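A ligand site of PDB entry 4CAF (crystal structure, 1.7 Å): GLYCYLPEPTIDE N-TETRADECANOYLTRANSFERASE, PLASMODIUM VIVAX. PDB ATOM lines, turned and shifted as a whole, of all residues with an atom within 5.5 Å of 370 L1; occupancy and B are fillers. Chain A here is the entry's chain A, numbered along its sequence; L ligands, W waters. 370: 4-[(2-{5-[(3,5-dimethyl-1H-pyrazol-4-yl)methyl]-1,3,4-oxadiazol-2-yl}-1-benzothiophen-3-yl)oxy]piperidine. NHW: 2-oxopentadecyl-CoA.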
ATOM      1  N   VAL A  70     -11.056  29.024  10.945  1.00  0.00           N
ATOM      2  CA  VAL A  70     -10.348  27.959  10.164  1.00  0.00           C
ATOM      3  C   VAL A  70     -10.891  26.559  10.400  1.00  0.00           C
ATOM      4  O   VAL A  70     -11.067  26.165  11.524  1.00  0.00           O
ATOM      5  CB  VAL A  70      -8.862  27.923  10.641  1.00  0.00           C
ATOM      6  CG1 VAL A  70      -8.126  26.831   9.884  1.00  0.00           C
ATOM      7  CG2 VAL A  70      -8.220  29.301  10.457  1.00  0.00           C
ATOM      8  N   GLU A  71     -11.107  25.797   9.314  1.00  0.00           N
ATOM      9  CA  GLU A  71     -11.430  24.365   9.472  1.00  0.00           C
ATOM     10  C   GLU A  71     -10.328  23.554   8.890  1.00  0.00           C
ATOM     11  O   GLU A  71      -9.496  24.080   8.135  1.00  0.00           O
ATOM     12  CB  GLU A  71     -12.731  24.019   8.660  1.00  0.00           C
ATOM     13  CG  GLU A  71     -13.896  24.841   9.172  1.00  0.00           C
ATOM     14  CD  GLU A  71     -15.206  24.642   8.355  1.00  0.00           C
ATOM     15  OE1 GLU A  71     -15.221  23.829   7.380  1.00  0.00           O
ATOM     16  OE2 GLU A  71     -16.215  25.300   8.729  1.00  0.00           O
ATOM     17  N   ASP A  72     -10.277  22.280   9.248  1.00  0.00           N
ATOM     18  CA  ASP A  72      -9.291  21.382   8.644  1.00  0.00           C
ATOM     19  C   ASP A  72      -9.729  21.115   7.205  1.00  0.00           C
ATOM     20  O   ASP A  72     -10.798  21.556   6.783  1.00  0.00           O
ATOM     21  CB  ASP A  72      -9.254  20.100   9.469  1.00  0.00           C
ATOM     22  CG  ASP A  72     -10.548  19.284   9.309  1.00  0.00           C
ATOM     23  OD1 ASP A  72     -11.649  19.788   9.651  1.00  0.00           O
ATOM     24  OD2 ASP A  72     -10.459  18.178   8.729  1.00  0.00           O
ATOM     25  N   PHE A  77     -13.409  19.682  11.603  1.00  0.00           N
ATOM     26  CA  PHE A  77     -13.069  20.415  12.851  1.00  0.00           C
ATOM     27  C   PHE A  77     -13.062  21.907  12.535  1.00  0.00           C
ATOM     28  O   PHE A  77     -12.629  22.281  11.456  1.00  0.00           O
ATOM     29  CB  PHE A  77     -11.633  19.990  13.283  1.00  0.00           C
ATOM     30  CG  PHE A  77     -11.584  18.554  13.716  1.00  0.00           C
ATOM     31  CD1 PHE A  77     -12.286  18.172  14.863  1.00  0.00           C
ATOM     32  CD2 PHE A  77     -10.966  17.569  12.918  1.00  0.00           C
ATOM     33  CE1 PHE A  77     -12.367  16.839  15.267  1.00  0.00           C
ATOM     34  CE2 PHE A  77     -11.017  16.239  13.332  1.00  0.00           C
ATOM     35  CZ  PHE A  77     -11.733  15.861  14.498  1.00  0.00           C
ATOM     36  N   ARG A  78     -13.510  22.778  13.437  1.00  0.00           N
ATOM     37  CA  ARG A  78     -13.279  24.195  13.179  1.00  0.00           C
ATOM     38  C   ARG A  78     -12.685  24.741  14.476  1.00  0.00           C
ATOM     39  O   ARG A  78     -13.178  24.444  15.554  1.00  0.00           O
ATOM     40  CB  ARG A  78     -14.611  24.920  12.904  1.00  0.00           C
ATOM     41  CG  ARG A  78     -14.346  26.423  12.633  1.00  0.00           C
ATOM     42  CD  ARG A  78     -15.586  27.254  12.335  1.00  0.00           C
ATOM     43  NE  ARG A  78     -16.457  26.594  11.407  1.00  0.00           N
ATOM     44  CZ  ARG A  78     -17.711  26.182  11.617  1.00  0.00           C
ATOM     45  NH1 ARG A  78     -18.442  26.461  12.701  1.00  0.00           N
ATOM     46  NH2 ARG A  78     -18.279  25.520  10.631  1.00  0.00           N
ATOM     47  N   PHE A  79     -11.633  25.542  14.408  1.00  0.00           N
ATOM     48  CA  PHE A  79     -11.087  26.054  15.659  1.00  0.00           C
ATOM     49  C   PHE A  79     -12.134  26.819  16.417  1.00  0.00           C
ATOM     50  O   PHE A  79     -12.991  27.481  15.818  1.00  0.00           O
ATOM     51  CB  PHE A  79      -9.923  27.068  15.376  1.00  0.00           C
ATOM     52  CG  PHE A  79      -8.652  26.473  14.903  1.00  0.00           C
ATOM     53  CD1 PHE A  79      -8.127  25.317  15.471  1.00  0.00           C
ATOM     54  CD2 PHE A  79      -7.855  27.195  13.990  1.00  0.00           C
ATOM     55  CE1 PHE A  79      -6.899  24.801  15.064  1.00  0.00           C
ATOM     56  CE2 PHE A  79      -6.615  26.658  13.535  1.00  0.00           C
ATOM     57  CZ  PHE A  79      -6.119  25.485  14.122  1.00  0.00           C
ATOM     58  N   TYR A  81     -11.429  29.021  19.456  1.00  0.00           N
ATOM     59  CA  TYR A  81     -10.737  29.870  20.455  1.00  0.00           C
ATOM     60  C   TYR A  81     -11.734  30.411  21.452  1.00  0.00           C
ATOM     61  O   TYR A  81     -12.759  30.930  21.061  1.00  0.00           O
ATOM     62  CB  TYR A  81     -10.127  31.077  19.726  1.00  0.00           C
ATOM     63  CG  TYR A  81      -8.962  30.758  18.832  1.00  0.00           C
ATOM     64  CD1 TYR A  81      -7.650  30.807  19.369  1.00  0.00           C
ATOM     65  CD2 TYR A  81      -9.123  30.443  17.476  1.00  0.00           C
ATOM     66  CE1 TYR A  81      -6.538  30.575  18.616  1.00  0.00           C
ATOM     67  CE2 TYR A  81      -7.987  30.151  16.706  1.00  0.00           C
ATOM     68  CZ  TYR A  81      -6.699  30.224  17.297  1.00  0.00           C
ATOM     69  OH  TYR A  81      -5.562  29.980  16.554  1.00  0.00           O
ATOM     70  N   ASN A 135      -3.130  38.116  13.130  1.00  0.00           N
ATOM     71  CA  ASN A 135      -3.841  36.853  13.390  1.00  0.00           C
ATOM     72  C   ASN A 135      -5.339  37.121  13.360  1.00  0.00           C
ATOM     73  O   ASN A 135      -5.771  38.282  13.340  1.00  0.00           O
ATOM     74  CB  ASN A 135      -3.438  36.332  14.768  1.00  0.00           C
ATOM     75  CG  ASN A 135      -3.509  34.828  14.887  1.00  0.00           C
ATOM     76  OD1 ASN A 135      -4.052  34.099  14.012  1.00  0.00           O
ATOM     77  ND2 ASN A 135      -2.908  34.334  15.935  1.00  0.00           N
ATOM     78  N   THR A 171       1.140  33.454  10.068  1.00  0.00           N
ATOM     79  CA  THR A 171       1.174  32.039   9.675  1.00  0.00           C
ATOM     80  C   THR A 171      -0.137  31.696   8.975  1.00  0.00           C
ATOM     81  O   THR A 171      -1.171  32.331   9.227  1.00  0.00           O
ATOM     82  CB  THR A 171       1.379  31.100  10.869  1.00  0.00           C
ATOM     83  OG1 THR A 171       0.375  31.265  11.889  1.00  0.00           O
ATOM     84  CG2 THR A 171       2.754  31.323  11.570  1.00  0.00           C
ATOM     85  N   TYR A 185       2.342  19.690  11.335  1.00  0.00           N
ATOM     86  CA  TYR A 185       1.962  19.366  12.701  1.00  0.00           C
ATOM     87  C   TYR A 185       1.754  17.895  12.920  1.00  0.00           C
ATOM     88  O   TYR A 185       1.449  17.147  11.960  1.00  0.00           O
ATOM     89  CB  TYR A 185       0.716  20.134  13.158  1.00  0.00           C
ATOM     90  CG  TYR A 185      -0.309  20.466  12.012  1.00  0.00           C
ATOM     91  CD1 TYR A 185      -1.289  19.531  11.649  1.00  0.00           C
ATOM     92  CD2 TYR A 185      -0.244  21.701  11.310  1.00  0.00           C
ATOM     93  CE1 TYR A 185      -2.210  19.839  10.634  1.00  0.00           C
ATOM     94  CE2 TYR A 185      -1.127  22.028  10.263  1.00  0.00           C
ATOM     95  CZ  TYR A 185      -2.099  21.061   9.951  1.00  0.00           C
ATOM     96  OH  TYR A 185      -3.024  21.341   8.979  1.00  0.00           O
ATOM     97  N   HIS A 187       0.482  14.909  16.087  1.00  0.00           N
ATOM     98  CA  HIS A 187      -0.533  14.796  17.162  1.00  0.00           C
ATOM     99  C   HIS A 187      -0.194  13.614  18.020  1.00  0.00           C
ATOM    100  O   HIS A 187       0.092  12.513  17.492  1.00  0.00           O
ATOM    101  CB  HIS A 187      -1.887  14.471  16.515  1.00  0.00           C
ATOM    102  CG  HIS A 187      -2.226  15.436  15.415  1.00  0.00           C
ATOM    103  ND1 HIS A 187      -2.650  16.715  15.698  1.00  0.00           N
ATOM    104  CD2 HIS A 187      -2.186  15.334  14.065  1.00  0.00           C
ATOM    105  CE1 HIS A 187      -2.824  17.375  14.550  1.00  0.00           C
ATOM    106  NE2 HIS A 187      -2.555  16.548  13.552  1.00  0.00           N
ATOM    107  N   PHE A 200     -10.839  11.047  13.946  1.00  0.00           N
ATOM    108  CA  PHE A 200      -9.432  11.536  14.011  1.00  0.00           C
ATOM    109  C   PHE A 200      -8.369  10.401  14.017  1.00  0.00           C
ATOM    110  O   PHE A 200      -7.308  10.520  13.407  1.00  0.00           O
ATOM    111  CB  PHE A 200      -9.339  12.429  15.239  1.00  0.00           C
ATOM    112  CG  PHE A 200      -8.079  13.296  15.331  1.00  0.00           C
ATOM    113  CD1 PHE A 200      -6.807  12.738  15.482  1.00  0.00           C
ATOM    114  CD2 PHE A 200      -8.178  14.704  15.370  1.00  0.00           C
ATOM    115  CE1 PHE A 200      -5.683  13.559  15.605  1.00  0.00           C
ATOM    116  CE2 PHE A 200      -7.052  15.519  15.500  1.00  0.00           C
ATOM    117  CZ  PHE A 200      -5.802  14.943  15.601  1.00  0.00           C
ATOM    118  N   TYR A 289      -0.759  25.840  25.054  1.00  0.00           N
ATOM    119  CA  TYR A 289      -2.005  26.649  25.197  1.00  0.00           C
ATOM    120  C   TYR A 289      -3.181  25.734  24.802  1.00  0.00           C
ATOM    121  O   TYR A 289      -3.000  24.698  24.100  1.00  0.00           O
ATOM    122  CB  TYR A 289      -1.977  27.955  24.376  1.00  0.00           C
ATOM    123  CG  TYR A 289      -1.706  27.871  22.855  1.00  0.00           C
ATOM    124  CD1 TYR A 289      -2.683  27.499  21.959  1.00  0.00           C
ATOM    125  CD2 TYR A 289      -0.440  28.226  22.350  1.00  0.00           C
ATOM    126  CE1 TYR A 289      -2.443  27.496  20.596  1.00  0.00           C
ATOM    127  CE2 TYR A 289      -0.174  28.216  20.961  1.00  0.00           C
ATOM    128  CZ  TYR A 289      -1.170  27.802  20.100  1.00  0.00           C
ATOM    129  OH  TYR A 289      -0.954  27.841  18.712  1.00  0.00           O
ATOM    130  N   LEU A 291      -6.523  25.119  22.646  1.00  0.00           N
ATOM    131  CA  LEU A 291      -7.228  25.576  21.470  1.00  0.00           C
ATOM    132  C   LEU A 291      -8.145  24.432  21.125  1.00  0.00           C
ATOM    133  O   LEU A 291      -7.745  23.532  20.397  1.00  0.00           O
ATOM    134  CB  LEU A 291      -6.246  25.915  20.342  1.00  0.00           C
ATOM    135  CG  LEU A 291      -6.899  26.267  18.981  1.00  0.00           C
ATOM    136  CD1 LEU A 291      -8.109  27.228  19.059  1.00  0.00           C
ATOM    137  CD2 LEU A 291      -5.809  26.888  18.048  1.00  0.00           C
ATOM    138  N   SER A 293     -11.147  22.419  19.194  1.00  0.00           N
ATOM    139  CA  SER A 293     -11.862  22.476  17.927  1.00  0.00           C
ATOM    140  C   SER A 293     -13.296  22.025  18.157  1.00  0.00           C
ATOM    141  O   SER A 293     -13.568  21.022  18.812  1.00  0.00           O
ATOM    142  CB  SER A 293     -11.213  21.614  16.851  1.00  0.00           C
ATOM    143  OG  SER A 293      -9.987  22.214  16.435  1.00  0.00           O
ATOM    144  N   LEU A 304     -13.421  18.995  20.633  1.00  0.00           N
ATOM    145  CA  LEU A 304     -12.148  18.275  20.818  1.00  0.00           C
ATOM    146  C   LEU A 304     -11.251  19.209  21.670  1.00  0.00           C
ATOM    147  O   LEU A 304     -11.040  20.331  21.241  1.00  0.00           O
ATOM    148  CB  LEU A 304     -11.484  18.032  19.485  1.00  0.00           C
ATOM    149  CG  LEU A 304     -10.048  17.433  19.496  1.00  0.00           C
ATOM    150  CD1 LEU A 304     -10.039  16.032  20.131  1.00  0.00           C
ATOM    151  CD2 LEU A 304      -9.445  17.339  18.119  1.00  0.00           C
ATOM    152  N   TYR A 308      -1.694  22.695  22.687  1.00  0.00           N
ATOM    153  CA  TYR A 308      -0.802  23.054  21.665  1.00  0.00           C
ATOM    154  C   TYR A 308       0.566  23.411  22.270  1.00  0.00           C
ATOM    155  O   TYR A 308       0.716  24.413  22.974  1.00  0.00           O
ATOM    156  CB  TYR A 308      -1.297  24.273  20.849  1.00  0.00           C
ATOM    157  CG  TYR A 308      -2.342  23.939  19.854  1.00  0.00           C
ATOM    158  CD1 TYR A 308      -3.567  23.392  20.290  1.00  0.00           C
ATOM    159  CD2 TYR A 308      -2.116  24.156  18.484  1.00  0.00           C
ATOM    160  CE1 TYR A 308      -4.572  23.016  19.370  1.00  0.00           C
ATOM    161  CE2 TYR A 308      -3.134  23.760  17.549  1.00  0.00           C
ATOM    162  CZ  TYR A 308      -4.353  23.187  18.029  1.00  0.00           C
ATOM    163  OH  TYR A 308      -5.338  22.812  17.119  1.00  0.00           O
ATOM    164  N   SER A 309       1.567  22.545  21.986  1.00  0.00           N
ATOM    165  CA  SER A 309       2.952  22.801  22.417  1.00  0.00           C
ATOM    166  C   SER A 309       3.396  24.187  22.030  1.00  0.00           C
ATOM    167  O   SER A 309       3.294  24.593  20.860  1.00  0.00           O
ATOM    168  CB  SER A 309       3.867  21.773  21.689  1.00  0.00           C
ATOM    169  OG  SER A 309       5.242  21.930  22.158  1.00  0.00           O
ATOM    170  N   ASN A 339      -0.797  18.545  20.506  1.00  0.00           N
ATOM    171  CA  ASN A 339      -0.417  18.874  19.104  1.00  0.00           C
ATOM    172  C   ASN A 339       0.900  19.618  19.168  1.00  0.00           C
ATOM    173  O   ASN A 339       1.101  20.491  20.073  1.00  0.00           O
ATOM    174  CB  ASN A 339      -1.451  19.779  18.446  1.00  0.00           C
ATOM    175  CG  ASN A 339      -2.815  19.073  18.277  1.00  0.00           C
ATOM    176  OD1 ASN A 339      -2.852  17.872  18.220  1.00  0.00           O
ATOM    177  ND2 ASN A 339      -3.901  19.831  18.109  1.00  0.00           N
ATOM    178  N   ALA A 340       1.770  19.334  18.211  1.00  0.00           N
ATOM    179  CA  ALA A 340       3.040  20.061  18.136  1.00  0.00           C
ATOM    180  C   ALA A 340       3.468  20.269  16.685  1.00  0.00           C
ATOM    181  O   ALA A 340       3.244  19.389  15.822  1.00  0.00           O
ATOM    182  CB  ALA A 340       4.129  19.284  18.866  1.00  0.00           C
ATOM    183  N   LEU A 341       4.162  21.374  16.400  1.00  0.00           N
ATOM    184  CA  LEU A 341       4.744  21.592  15.097  1.00  0.00           C
ATOM    185  C   LEU A 341       6.192  21.050  15.115  1.00  0.00           C
ATOM    186  O   LEU A 341       6.849  20.991  16.192  1.00  0.00           O
ATOM    187  CB  LEU A 341       4.901  23.120  14.872  1.00  0.00           C
ATOM    188  CG  LEU A 341       3.506  23.815  14.720  1.00  0.00           C
ATOM    189  CD1 LEU A 341       3.610  25.370  14.760  1.00  0.00           C
ATOM    190  CD2 LEU A 341       2.875  23.411  13.381  1.00  0.00           C
ATOM    191  N   LEU A 362       1.817  24.230   8.682  1.00  0.00           N
ATOM    192  CA  LEU A 362       1.675  25.686   8.908  1.00  0.00           C
ATOM    193  C   LEU A 362       2.858  26.425   8.271  1.00  0.00           C
ATOM    194  O   LEU A 362       4.035  26.152   8.612  1.00  0.00           O
ATOM    195  CB  LEU A 362       1.629  25.946  10.424  1.00  0.00           C
ATOM    196  CG  LEU A 362       1.180  27.334  10.794  1.00  0.00           C
ATOM    197  CD1 LEU A 362      -0.347  27.586  10.542  1.00  0.00           C
ATOM    198  CD2 LEU A 362       1.559  27.635  12.276  1.00  0.00           C
ATOM    199  N   VAL A 382       6.330  30.242  17.996  1.00  0.00           N
ATOM    200  CA  VAL A 382       5.035  29.517  17.848  1.00  0.00           C
ATOM    201  C   VAL A 382       3.917  30.559  18.003  1.00  0.00           C
ATOM    202  O   VAL A 382       3.882  31.224  19.062  1.00  0.00           O
ATOM    203  CB  VAL A 382       4.891  28.394  18.894  1.00  0.00           C
ATOM    204  CG1 VAL A 382       3.446  27.771  18.843  1.00  0.00           C
ATOM    205  CG2 VAL A 382       5.960  27.329  18.650  1.00  0.00           C
ATOM    206  N   LEU A 383       3.142  30.802  16.925  1.00  0.00           N
ATOM    207  CA  LEU A 383       2.047  31.773  16.985  1.00  0.00           C
ATOM    208  C   LEU A 383       0.789  31.103  17.577  1.00  0.00           C
ATOM    209  O   LEU A 383       0.799  29.906  17.837  1.00  0.00           O
ATOM    210  CB  LEU A 383       1.781  32.333  15.582  1.00  0.00           C
ATOM    211  CG  LEU A 383       2.891  33.213  14.978  1.00  0.00           C
ATOM    212  CD1 LEU A 383       2.424  34.100  13.825  1.00  0.00           C
ATOM    213  CD2 LEU A 383       3.502  34.024  16.084  1.00  0.00           C
ATOM    214  N   LEU A 384      -0.269  31.907  17.779  1.00  0.00           N
ATOM    215  CA  LEU A 384      -1.489  31.431  18.370  1.00  0.00           C
ATOM    216  C   LEU A 384      -2.515  31.013  17.365  1.00  0.00           C
ATOM    217  O   LEU A 384      -2.515  31.433  16.196  1.00  0.00           O
ATOM    218  CB  LEU A 384      -2.043  32.591  19.198  1.00  0.00           C
ATOM    219  CG  LEU A 384      -1.042  33.106  20.213  1.00  0.00           C
ATOM    220  CD1 LEU A 384      -1.772  34.154  21.078  1.00  0.00           C
ATOM    221  CD2 LEU A 384      -0.562  31.974  21.082  1.00  0.00           C
ATOM    222  OXT LEU A 384      -3.396  30.249  17.802  1.00  0.00           O
HETATM  223  C   370 L   1      -8.449  23.438  12.196  1.00  0.00           C
HETATM  224  N   370 L   1      -3.985  24.441  11.566  1.00  0.00           N
HETATM  225  O   370 L   1      -3.387  22.904  13.145  1.00  0.00           O
HETATM  226  S   370 L   1      -1.102  22.534  14.939  1.00  0.00           S
HETATM  227  C1  370 L   1      -7.722  22.398  13.035  1.00  0.00           C
HETATM  228  N1  370 L   1      -2.872  24.918  12.280  1.00  0.00           N
HETATM  229  O1  370 L   1      -1.160  26.379  14.428  1.00  0.00           O
HETATM  230  C2  370 L   1      -6.325  21.936  12.798  1.00  0.00           C
HETATM  231  N2  370 L   1      -2.625  29.470  14.078  1.00  0.00           N
HETATM  232  C3  370 L   1      -5.441  22.405  11.658  1.00  0.00           C
HETATM  233  N3  370 L   1      -7.195  20.852  14.622  1.00  0.00           N
HETATM  234  C4  370 L   1      -4.283  23.242  12.096  1.00  0.00           C
HETATM  235  N4  370 L   1      -8.173  21.741  14.127  1.00  0.00           N
HETATM  236  C5  370 L   1      -2.551  23.946  13.109  1.00  0.00           C
HETATM  237  C6  370 L   1      -1.528  23.945  14.139  1.00  0.00           C
HETATM  238  C7  370 L   1      -0.924  25.112  14.831  1.00  0.00           C
HETATM  239  C8  370 L   1      -1.582  27.255  15.517  1.00  0.00           C
HETATM  240  C9  370 L   1      -3.112  27.491  15.507  1.00  0.00           C
HETATM  241  C10 370 L   1      -3.509  28.299  14.242  1.00  0.00           C
HETATM  242  C11 370 L   1      -1.185  29.302  14.128  1.00  0.00           C
HETATM  243  C12 370 L   1      -0.791  28.561  15.398  1.00  0.00           C
HETATM  244  C13 370 L   1      -0.050  24.727  15.978  1.00  0.00           C
HETATM  245  C14 370 L   1       0.789  25.516  16.865  1.00  0.00           C
HETATM  246  C15 370 L   1       1.512  24.814  17.851  1.00  0.00           C
HETATM  247  C16 370 L   1       1.446  23.410  17.989  1.00  0.00           C
HETATM  248  C17 370 L   1       0.666  22.575  17.102  1.00  0.00           C
HETATM  249  C18 370 L   1      -0.047  23.232  16.061  1.00  0.00           C
HETATM  250  C19 370 L   1      -6.083  20.951  13.875  1.00  0.00           C
HETATM  251  C20 370 L   1      -4.855  20.153  14.164  1.00  0.00           C
HETATM  252  S1  NHW L   2      -4.372  32.134   8.871  1.00  0.00           S
HETATM  253  C2  NHW L   2      -6.216  31.997   9.119  1.00  0.00           C
HETATM  254  C3  NHW L   2      -6.924  32.874   8.094  1.00  0.00           C
HETATM  255  N4  NHW L   2      -8.404  32.748   8.389  1.00  0.00           N
HETATM  256  C5  NHW L   2      -9.090  31.724   7.949  1.00  0.00           C
HETATM  257  O5  NHW L   2      -8.600  30.804   7.251  1.00  0.00           O
HETATM  258  C6  NHW L   2     -10.522  31.818   8.399  1.00  0.00           C
HETATM  259  C7  NHW L   2     -11.573  31.143   7.391  1.00  0.00           C
HETATM  260  N8  NHW L   2     -11.343  31.839   6.101  1.00  0.00           N
HETATM  261  C9  NHW L   2     -11.748  33.106   5.938  1.00  0.00           C
HETATM  262  O9  NHW L   2     -12.296  33.747   6.852  1.00  0.00           O
HETATM  263  CP  NHW L   2      -3.976  33.091  10.423  1.00  0.00           C
HETATM  264  C10 NHW L   2     -11.535  33.687   4.578  1.00  0.00           C
HETATM  265  O10 NHW L   2     -11.319  32.575   3.640  1.00  0.00           O
HETATM  266  C11 NHW L   2     -10.323  34.633   4.507  1.00  0.00           C
HETATM  267  C12 NHW L   2     -10.048  35.064   3.044  1.00  0.00           C
HETATM  268  C13 NHW L   2      -8.991  33.932   4.938  1.00  0.00           C
HETATM  269  C14 NHW L   2     -10.604  35.920   5.357  1.00  0.00           C
HETATM  270  N1A NHW L   2      -3.684  35.129   4.607  1.00  0.00           N
HETATM  271  O1A NHW L   2     -11.806  37.059  -1.991  1.00  0.00           O
HETATM  272  P1A NHW L   2     -11.170  37.120  -0.657  1.00  0.00           P
HETATM  273  C1M NHW L   2      -4.107  34.610  10.108  1.00  0.00           C
HETATM  274  O1M NHW L   2      -5.172  35.158  10.331  1.00  0.00           O
HETATM  275  C1X NHW L   2      -5.812  35.998   0.008  1.00  0.00           C
HETATM  276  C2A NHW L   2      -3.430  36.064   3.682  1.00  0.00           C
HETATM  277  O2A NHW L   2     -11.657  38.081   0.346  1.00  0.00           O
HETATM  278  P2A NHW L   2     -11.894  35.040   1.115  1.00  0.00           P
HETATM  279  C2M NHW L   2      -2.997  35.357   9.294  1.00  0.00           C
HETATM  280  C2X NHW L   2      -5.968  35.136  -1.233  1.00  0.00           C
HETATM  281  O2X NHW L   2      -4.695  34.553  -1.642  1.00  0.00           O
HETATM  282  N3A NHW L   2      -4.079  36.181   2.505  1.00  0.00           N
HETATM  283  O3A NHW L   2     -11.011  35.689  -0.015  1.00  0.00           O
HETATM  284  C3M NHW L   2      -3.653  36.509   8.402  1.00  0.00           C
HETATM  285  C3X NHW L   2      -6.428  36.184  -2.247  1.00  0.00           C
HETATM  286  O3X NHW L   2      -5.332  36.983  -2.730  1.00  0.00           O
HETATM  287  P3X NHW L   2      -4.683  36.684  -4.162  1.00  0.00           P
HETATM  288  C4A NHW L   2      -5.087  35.309   2.230  1.00  0.00           C
HETATM  289  O4A NHW L   2     -13.299  35.504   1.181  1.00  0.00           O
HETATM  290  C4M NHW L   2      -2.569  37.149   7.581  1.00  0.00           C
HETATM  291  C4X NHW L   2      -7.293  37.131  -1.385  1.00  0.00           C
HETATM  292  O4X NHW L   2      -6.993  36.747   0.002  1.00  0.00           O
HETATM  293  C5A NHW L   2      -5.397  34.293   3.152  1.00  0.00           C
HETATM  294  O5A NHW L   2     -11.626  33.554   1.037  1.00  0.00           O
HETATM  295  C5M NHW L   2      -3.104  38.140   6.562  1.00  0.00           C
HETATM  296  C5X NHW L   2      -8.768  36.661  -1.606  1.00  0.00           C
HETATM  297  O5X NHW L   2      -9.597  37.491  -0.801  1.00  0.00           O
HETATM  298  C6A NHW L   2      -4.697  34.203   4.355  1.00  0.00           C
HETATM  299  N6A NHW L   2      -4.930  33.268   5.289  1.00  0.00           N
HETATM  300  O6A NHW L   2     -11.265  35.595   2.465  1.00  0.00           O
HETATM  301  C6M NHW L   2      -2.003  38.902   5.789  1.00  0.00           C
HETATM  302  N7A NHW L   2      -6.424  33.593   2.602  1.00  0.00           N
HETATM  303  O7A NHW L   2      -3.369  37.440  -4.261  1.00  0.00           O
HETATM  304  C7M NHW L   2      -1.252  39.926   6.740  1.00  0.00           C
HETATM  305  C8A NHW L   2      -6.722  34.109   1.396  1.00  0.00           C
HETATM  306  O8A NHW L   2      -4.290  35.187  -4.157  1.00  0.00           O
HETATM  307  C8M NHW L   2      -0.068  40.538   5.993  1.00  0.00           C
HETATM  308  N9A NHW L   2      -5.868  35.145   1.162  1.00  0.00           N
HETATM  309  O9A NHW L   2      -5.672  36.958  -5.246  1.00  0.00           O
HETATM  310  C9M NHW L   2       0.713  41.511   6.933  1.00  0.00           C
HETATM  311  CAM NHW L   2      -0.130  42.789   7.135  1.00  0.00           C
HETATM  312  CBM NHW L   2       0.523  43.900   7.982  1.00  0.00           C
HETATM  313  CCM NHW L   2       1.870  44.472   7.379  1.00  0.00           C
HETATM  314  CDM NHW L   2       2.430  45.538   8.396  1.00  0.00           C
HETATM  315  CEM NHW L   2       3.768  46.149   7.855  1.00  0.00           C
HETATM  316  O   HOH W   1      -5.210  31.529  14.230  1.00  0.00           O
HETATM  317  O   HOH W   2      -6.663  19.485  17.335  1.00  0.00           O
HETATM  318  O   HOH W   3      -4.459  25.666   9.161  1.00  0.00           O
HETATM  319  O   HOH W   4       4.778  23.343  18.541  1.00  0.00           O
HETATM  320  O   HOH W   5      -2.632  30.130  11.290  1.00  0.00           O
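O of Leu 384 lies within salt-bridge range of N2 of 370 L1 (2.9 Å).
The side-chain hydroxyl of Ser 293 sits at hydrogen-bond distance from a nitrogen (N4) of 370 L1 (3.0 Å).
The backbone NH of Tyr 308 is in hydrogen-bond range of the backbone carbonyl oxygen of Tyr 289, at 2.8 Å.
N of Ser 309 sits at hydrogen-bond distance from O of Asn 339 (2.8 Å).
The side-chain carboxylate (OE2) of Glu 71 is in salt-bridge range of the guanidinium group (NH2) of Arg 78, at 2.8 Å.
N of Phe 79 sits at hydrogen-bond distance from O of Val 70 (3.0 Å).
The chain-end carboxylate of Leu 384 is in hydrogen-bond range of the side-chain amide nitrogen of Asn 135.
A ring nitrogen (ND1) of His 187 is in hydrogen-bond range of the side-chain amide oxygen of Asn 339 (2.8 Å).
The side-chain hydroxyl of Tyr 289 lies within hydrogen-bond range of the backbone carbonyl oxygen of Leu 383 (2.8 Å).
The backbone carbonyl oxygen of Ser 293 is in hydrogen-bond range of the backbone NH of Leu 304 (2.7 Å).
Val 70 touches 370 L1 (O to C, 3.8 Å).
C of Glu 71 touches C of 370 L1, at 3.8 Å.
Asp 72 touches 370 L1 (N to C, 3.7 Å).
Phe 77 touches 370 L1 (CB to N4, 3.97 Å).
Phe 79 touches 370 L1 (CE1 to C1, 3.3 Å).
OH of Tyr 81 touches C10 of 370 L1, 3.5 Å away.
Thr 171 touches 370 L1.
CB of Tyr 185 touches S of 370 L1, at 3.5 Å.
CE1 of His 187 touches C20 of 370 L1, at 3.5 Å.
Tyr 289 touches 370 L1 (OH to C8, 3.3 Å).
Leu 291 touches 370 L1.
Tyr 308 touches 370 L1 (CD2 to C13, 3.3 Å).
Ser 309 touches 370 L1 (O to C15, 3.5 Å).
O of Asn 339 touches C16 of 370 L1 (3.6 Å).
Ala 340 touches 370 L1.
Leu 341 touches 370 L1 (CD1 to C14, 3.5 Å).
Leu 362 touches 370 L1.
CG1 of Val 382 touches C15 of 370 L1 (3.7 Å).
Leu 383 touches 370 L1 (O to C12, 3.2 Å).
21 residues have an atom within 4 Å of 370 L1: Val 70, Glu 71, Asp 72, Phe 77, Phe 79, Tyr 81, Thr 171, Tyr 185, His 187, Tyr 289, Leu 291, Ser 293, Tyr 308, Ser 309, Asn 339, Ala 340, Leu 341, Leu 362, Val 382, Leu 383 and Leu 384.
Along chain A the residues within 4 Å of 370 L1 span positions 70 to 384.
The nearest printed residue that does not touch 370 L1 is Asn 135 (4.8 Å).
Water W5 lies within hydrogen-bond range of N2 of 370 L1, OG1 of Thr 171 and S1 of NHW L2.
Water W2 lies within hydrogen-bond range of the side-chain amide nitrogen (ND2) of Asn 339 (2.9 Å) and a nitrogen (N3) of 370 L1 (3.1 Å).
Water W1 lies within hydrogen-bond range of the side-chain hydroxyl (OH) of Tyr 81 (2.8 Å), the side-chain amide oxygen (OD1) of Asn 135 (2.8 Å), a nitrogen (N2) of 370 L1 (3.3 Å) and the chain-end carboxylate (O) of Leu 384 (3.3 Å).
Water W4 lies within hydrogen-bond range of N of Leu 341 (3.0 Å) and O of Ser 309 (3.0 Å).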
